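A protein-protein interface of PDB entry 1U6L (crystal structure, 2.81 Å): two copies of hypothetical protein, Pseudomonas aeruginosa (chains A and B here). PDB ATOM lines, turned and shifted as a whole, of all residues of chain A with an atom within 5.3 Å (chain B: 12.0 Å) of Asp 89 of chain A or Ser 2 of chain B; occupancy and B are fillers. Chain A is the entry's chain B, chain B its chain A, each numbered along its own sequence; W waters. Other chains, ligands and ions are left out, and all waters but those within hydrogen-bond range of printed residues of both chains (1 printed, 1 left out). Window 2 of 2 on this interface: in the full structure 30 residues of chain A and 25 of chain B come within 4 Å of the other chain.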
ATOM      1  N   PHE A  63      -9.312   6.932 -16.001  1.00  0.00           N
ATOM      2  CA  PHE A  63      -8.369   6.390 -17.011  1.00  0.00           C
ATOM      3  C   PHE A  63      -8.616   4.934 -17.477  1.00  0.00           C
ATOM      4  O   PHE A  63      -9.327   4.208 -16.825  1.00  0.00           O
ATOM      5  CB  PHE A  63      -6.981   6.506 -16.396  1.00  0.00           C
ATOM      6  CG  PHE A  63      -6.574   7.859 -16.262  1.00  0.00           C
ATOM      7  CD1 PHE A  63      -6.697   8.496 -15.083  1.00  0.00           C
ATOM      8  CD2 PHE A  63      -6.193   8.586 -17.418  1.00  0.00           C
ATOM      9  CE1 PHE A  63      -6.385   9.869 -14.957  1.00  0.00           C
ATOM     10  CE2 PHE A  63      -5.840   9.986 -17.336  1.00  0.00           C
ATOM     11  CZ  PHE A  63      -5.941  10.640 -16.069  1.00  0.00           C
ATOM     12  N   ASN A  87       1.120   8.051 -12.532  1.00  0.00           N
ATOM     13  CA  ASN A  87       1.436   9.155 -11.601  1.00  0.00           C
ATOM     14  C   ASN A  87       0.575   9.006 -10.443  1.00  0.00           C
ATOM     15  O   ASN A  87      -0.630   8.915 -10.632  1.00  0.00           O
ATOM     16  CB  ASN A  87       1.165  10.499 -12.204  1.00  0.00           C
ATOM     17  CG  ASN A  87       1.835  10.606 -13.494  1.00  0.00           C
ATOM     18  OD1 ASN A  87       2.943  10.078 -13.649  1.00  0.00           O
ATOM     19  ND2 ASN A  87       1.178  11.202 -14.488  1.00  0.00           N
ATOM     20  N   VAL A  88       1.161   8.980  -9.246  1.00  0.00           N
ATOM     21  CA  VAL A  88       0.392   8.950  -8.019  1.00  0.00           C
ATOM     22  C   VAL A  88       0.983   9.787  -6.886  1.00  0.00           C
ATOM     23  O   VAL A  88       2.012  10.385  -7.019  1.00  0.00           O
ATOM     24  CB  VAL A  88       0.059   7.496  -7.635  1.00  0.00           C
ATOM     25  CG1 VAL A  88       1.330   6.725  -7.253  1.00  0.00           C
ATOM     26  CG2 VAL A  88      -1.066   7.458  -6.575  1.00  0.00           C
ATOM     27  N   ASP A  89       0.280   9.831  -5.772  1.00  0.00           N
ATOM     28  CA  ASP A  89       0.403  10.847  -4.698  1.00  0.00           C
ATOM     29  C   ASP A  89       1.455  10.486  -3.650  1.00  0.00           C
ATOM     30  O   ASP A  89       2.032  11.344  -3.014  1.00  0.00           O
ATOM     31  CB  ASP A  89      -0.948  10.984  -3.969  1.00  0.00           C
ATOM     32  CG  ASP A  89      -2.004  11.709  -4.799  1.00  0.00           C
ATOM     33  OD1 ASP A  89      -3.000  12.223  -4.227  1.00  0.00           O
ATOM     34  OD2 ASP A  89      -1.846  11.779  -6.033  1.00  0.00           O
ATOM     35  N   SER A  90       1.676   9.204  -3.451  1.00  0.00           N
ATOM     36  CA  SER A  90       2.505   8.799  -2.386  1.00  0.00           C
ATOM     37  C   SER A  90       3.798   8.134  -2.922  1.00  0.00           C
ATOM     38  O   SER A  90       3.808   7.345  -3.919  1.00  0.00           O
ATOM     39  CB  SER A  90       1.704   7.837  -1.496  1.00  0.00           C
ATOM     40  OG  SER A  90       2.422   7.440  -0.343  1.00  0.00           O
ATOM     41  N   LYS A  91       4.872   8.425  -2.197  1.00  0.00           N
ATOM     42  CA  LYS A  91       6.119   7.739  -2.309  1.00  0.00           C
ATOM     43  C   LYS A  91       5.878   6.272  -1.916  1.00  0.00           C
ATOM     44  O   LYS A  91       6.634   5.417  -2.322  1.00  0.00           O
ATOM     45  CB  LYS A  91       7.040   8.400  -1.326  1.00  0.00           C
ATOM     46  CG  LYS A  91       8.368   8.864  -1.828  1.00  0.00           C
ATOM     47  N   GLU A  93       2.936   4.659  -2.518  1.00  0.00           N
ATOM     48  CA  GLU A  93       2.163   4.102  -3.628  1.00  0.00           C
ATOM     49  C   GLU A  93       3.119   3.791  -4.808  1.00  0.00           C
ATOM     50  O   GLU A  93       3.068   2.657  -5.383  1.00  0.00           O
ATOM     51  CB  GLU A  93       0.910   4.912  -3.986  1.00  0.00           C
ATOM     52  N   CYS A 135       5.950  10.069  -8.785  1.00  0.00           N
ATOM     53  CA  CYS A 135       5.333  10.586  -7.597  1.00  0.00           C
ATOM     54  C   CYS A 135       5.905  11.942  -7.488  1.00  0.00           C
ATOM     55  O   CYS A 135       6.955  12.142  -7.985  1.00  0.00           O
ATOM     56  CB  CYS A 135       5.828   9.820  -6.413  1.00  0.00           C
ATOM     57  SG  CYS A 135       5.060  10.528  -5.042  1.00  0.00           S
ATOM     58  N   GLU A 136       5.280  12.870  -6.793  1.00  0.00           N
ATOM     59  CA  GLU A 136       5.892  14.176  -6.675  1.00  0.00           C
ATOM     60  C   GLU A 136       5.523  14.951  -5.374  1.00  0.00           C
ATOM     61  O   GLU A 136       5.525  16.192  -5.359  1.00  0.00           O
ATOM     62  CB  GLU A 136       5.615  14.946  -7.978  1.00  0.00           C
ATOM     63  N   GLN A 137       5.234  14.230  -4.277  1.00  0.00           N
ATOM     64  CA  GLN A 137       4.844  14.894  -3.006  1.00  0.00           C
ATOM     65  C   GLN A 137       5.307  14.270  -1.647  1.00  0.00           C
ATOM     66  O   GLN A 137       6.384  14.575  -1.125  1.00  0.00           O
ATOM     67  CB  GLN A 137       3.329  15.185  -2.993  1.00  0.00           C
ATOM     68  N   ASP A 138       4.457  13.429  -1.074  1.00  0.00           N
ATOM     69  CA  ASP A 138       4.681  12.844   0.231  1.00  0.00           C
ATOM     70  C   ASP A 138       5.568  11.609   0.148  1.00  0.00           C
ATOM     71  O   ASP A 138       5.100  10.484   0.388  1.00  0.00           O
ATOM     72  CB  ASP A 138       3.334  12.518   0.903  1.00  0.00           C
ATOM     73  N   SER B   2      -6.651  11.550  -8.536  1.00  0.00           N
ATOM     74  CA  SER B   2      -5.585  10.509  -8.249  1.00  0.00           C
ATOM     75  C   SER B   2      -5.303   9.337  -9.230  1.00  0.00           C
ATOM     76  O   SER B   2      -6.119   8.963 -10.072  1.00  0.00           O
ATOM     77  CB  SER B   2      -5.725   9.949  -6.849  1.00  0.00           C
ATOM     78  OG  SER B   2      -4.444   9.514  -6.444  1.00  0.00           O
ATOM     79  N   LEU B   3      -4.120   8.759  -9.078  1.00  0.00           N
ATOM     80  CA  LEU B   3      -3.620   7.762  -9.981  1.00  0.00           C
ATOM     81  C   LEU B   3      -3.871   8.047 -11.444  1.00  0.00           C
ATOM     82  O   LEU B   3      -4.883   7.665 -11.955  1.00  0.00           O
ATOM     83  CB  LEU B   3      -4.390   6.561  -9.733  1.00  0.00           C
ATOM     84  CG  LEU B   3      -3.674   5.293 -10.266  1.00  0.00           C
ATOM     85  CD1 LEU B   3      -4.667   4.021  -9.896  1.00  0.00           C
ATOM     86  CD2 LEU B   3      -3.138   5.380 -11.751  1.00  0.00           C
ATOM     87  N   GLN B   4      -2.922   8.666 -12.119  1.00  0.00           N
ATOM     88  CA  GLN B   4      -3.117   9.152 -13.455  1.00  0.00           C
ATOM     89  C   GLN B   4      -2.365   8.209 -14.360  1.00  0.00           C
ATOM     90  O   GLN B   4      -1.159   7.988 -14.132  1.00  0.00           O
ATOM     91  CB  GLN B   4      -2.421  10.477 -13.548  1.00  0.00           C
ATOM     92  CG  GLN B   4      -2.975  11.573 -12.729  1.00  0.00           C
ATOM     93  CD  GLN B   4      -3.234  12.765 -13.615  1.00  0.00           C
ATOM     94  OE1 GLN B   4      -2.312  13.382 -14.208  1.00  0.00           O
ATOM     95  NE2 GLN B   4      -4.516  13.073 -13.766  1.00  0.00           N
ATOM     96  N   ILE B   5      -3.008   7.598 -15.360  1.00  0.00           N
ATOM     97  CA  ILE B   5      -2.194   6.804 -16.287  1.00  0.00           C
ATOM     98  C   ILE B   5      -2.143   7.591 -17.556  1.00  0.00           C
ATOM     99  O   ILE B   5      -3.177   8.012 -18.054  1.00  0.00           O
ATOM    100  CB  ILE B   5      -2.539   5.301 -16.471  1.00  0.00           C
ATOM    101  CG1 ILE B   5      -3.163   5.050 -17.798  1.00  0.00           C
ATOM    102  CG2 ILE B   5      -3.466   4.786 -15.411  1.00  0.00           C
ATOM    103  CD1 ILE B   5      -4.588   5.072 -17.642  1.00  0.00           C
ATOM    104  N   VAL B   6      -0.918   7.856 -18.027  1.00  0.00           N
ATOM    105  CA  VAL B   6      -0.653   8.618 -19.260  1.00  0.00           C
ATOM    106  C   VAL B   6       0.341   7.902 -20.183  1.00  0.00           C
ATOM    107  O   VAL B   6       1.383   7.544 -19.693  1.00  0.00           O
ATOM    108  CB  VAL B   6      -0.059   9.931 -18.802  1.00  0.00           C
ATOM    109  CG1 VAL B   6       0.701  10.625 -19.956  1.00  0.00           C
ATOM    110  CG2 VAL B   6      -1.196  10.777 -18.143  1.00  0.00           C
ATOM    111  N   ARG B  57       4.559  17.810 -22.961  1.00  0.00           N
ATOM    112  CA  ARG B  57       3.325  17.368 -22.287  1.00  0.00           C
ATOM    113  C   ARG B  57       2.167  18.079 -22.921  1.00  0.00           C
ATOM    114  O   ARG B  57       2.212  19.301 -23.038  1.00  0.00           O
ATOM    115  CB  ARG B  57       3.398  17.650 -20.811  1.00  0.00           C
ATOM    116  CG  ARG B  57       2.161  17.363 -20.092  1.00  0.00           C
ATOM    117  CD  ARG B  57       2.373  17.582 -18.543  1.00  0.00           C
ATOM    118  NE  ARG B  57       1.317  16.967 -17.744  1.00  0.00           N
ATOM    119  CZ  ARG B  57       1.018  15.659 -17.802  1.00  0.00           C
ATOM    120  NH1 ARG B  57       1.672  14.827 -18.612  1.00  0.00           N
ATOM    121  NH2 ARG B  57       0.056  15.152 -17.054  1.00  0.00           N
ATOM    122  N   SER B  62      -8.871  16.037 -19.511  1.00  0.00           N
ATOM    123  CA  SER B  62      -8.308  15.379 -18.355  1.00  0.00           C
ATOM    124  C   SER B  62      -7.378  14.225 -18.803  1.00  0.00           C
ATOM    125  O   SER B  62      -6.834  13.480 -17.994  1.00  0.00           O
ATOM    126  CB  SER B  62      -9.465  14.834 -17.517  1.00  0.00           C
ATOM    127  OG  SER B  62      -9.993  13.716 -18.214  1.00  0.00           O
ATOM    128  N   PHE B  63      -7.180  14.068 -20.101  1.00  0.00           N
ATOM    129  CA  PHE B  63      -6.075  13.142 -20.532  1.00  0.00           C
ATOM    130  C   PHE B  63      -4.728  13.826 -20.912  1.00  0.00           C
ATOM    131  O   PHE B  63      -4.682  15.062 -21.095  1.00  0.00           O
ATOM    132  CB  PHE B  63      -6.597  12.257 -21.658  1.00  0.00           C
ATOM    133  CG  PHE B  63      -7.787  11.488 -21.269  1.00  0.00           C
ATOM    134  CD1 PHE B  63      -9.027  12.156 -21.091  1.00  0.00           C
ATOM    135  CD2 PHE B  63      -7.672  10.129 -20.997  1.00  0.00           C
ATOM    136  CE1 PHE B  63     -10.186  11.463 -20.686  1.00  0.00           C
ATOM    137  CE2 PHE B  63      -8.813   9.394 -20.631  1.00  0.00           C
ATOM    138  CZ  PHE B  63     -10.079  10.054 -20.455  1.00  0.00           C
ATOM    139  N   ALA B  64      -3.670  13.048 -21.012  1.00  0.00           N
ATOM    140  CA  ALA B  64      -2.393  13.659 -21.323  1.00  0.00           C
ATOM    141  C   ALA B  64      -1.580  12.720 -22.166  1.00  0.00           C
ATOM    142  O   ALA B  64      -1.595  11.549 -21.878  1.00  0.00           O
ATOM    143  CB  ALA B  64      -1.586  14.140 -20.075  1.00  0.00           C
HETATM  144  O   HOH W   1       0.214  13.406 -15.276  1.00  0.00           O
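Hydrophobic or aromatic side chains of chain B that line the printed part of chain A: Ile 5.
Along chain B the printed residues that touch a printed residue of chain A span positions 2 to 62.
Printed residues of chain A that touch a printed residue of chain B: Phe 63, Asn 87, Val 88 and Asp 89.
Hydrophobic or aromatic side chains of chain A within 4 Å of the printed part of chain B: Phe 63 and Val 88.
Along chain A the printed residues that touch a printed residue of chain B span positions 63 to 89.
Among the printed residues, 8 pairs touch across the chains.
Among the printed residues, no Asp or Glu carboxylate lies within 4 Å of a Lys or Arg side-chain nitrogen of the other chain.
Position printed for both chains: 63.
The backbone carbonyl oxygen of Val 88 of chain A lies close to the side-chain sulfur of Cys 135 of chain A, 3.6 Å away.
The side-chain sulfur (SG) of Cys 135 of chain A lies within hydrogen-bond range of the backbone carbonyl oxygen (O) of Asp 89 of chain A (3.7 Å).
Water W1 lies within hydrogen-bond range of NH2 of Arg 57 of chain B (2.5 Å), ND2 of Asn 87 of chain A (2.5 Å) and OE1 of Gln 4 of chain B (2.7 Å).
Leu 3 of chain B touches Phe 63 of chain A.
CZ of Phe 63 of chain A touches NE2 of Gln 4 of chain B, 3.6 Å away.
Ile 5 of chain B touches Phe 63 of chain A (CD1 to CB, 3.1 Å).
Phe 63 of chain A touches Ser 62 of chain B.
Asn 87 of chain A touches Leu 3 of chain B.
Val 88 of chain A touches Ser 2 of chain B (CG2 to OG, 3.96 Å).
OD2 of Asp 89 of chain A sits at hydrogen-bond distance from OG of Ser 2 of chain B, 3.5 Å away.
N of Gln 4 of chain B is in hydrogen-bond range of O of Asn 87 of chain A (2.7 Å).
Of the printed residues of chain B, Phe 63 of chain A touches Leu 3 (3.7 Å), Gln 4 (3.6 Å), Ile 5 (3.1 Å) and Ser 62 (3.5 Å).
Val 88 of chain A touches just one residue of chain B: Ser 2 (3.96 Å).
Asp 89 of chain A touches just one residue of chain B: Ser 2.
No residue of chain B comes within 4 Å of Ser 90 of chain A.
No residue of chain B comes within 4 Å of Lys 91 of chain A.
Glu 93 of chain A touches none of the printed residues of chain B.
No residue of chain B comes within 4 Å of Cys 135 of chain A.
Gln 137 of chain A touches none of the printed residues of chain B.
No residue of chain B comes within 4 Å of Asp 138 of chain A.
Of the printed residues of chain A, Ser 2 of chain B touches Val 88 and Asp 89.
Of the printed residues of chain A, Leu 3 of chain B touches Phe 63 (3.7 Å) and Asn 87 (3.3 Å).
Printed residues of chain A within 4 Å of Gln 4 of chain B: Phe 63 and Asn 87.
Printed residues of chain A within 4 Å of Ile 5 of chain B: Phe 63 (3.1 Å).
Arg 57 of chain B touches none of the printed residues of chain A.
Printed residues of chain A within 4 Å of Ser 62 of chain B: Phe 63 (3.5 Å).
Ala 64 of chain B touches none of the printed residues of chain A.
The nearest residue of chain B that does not touch Asp 89 of chain A is Leu 3 of chain B (4.9 Å).
The nearest residue of chain A that does not touch Ser 2 of chain B is Asn 87 of chain A (4.9 Å).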
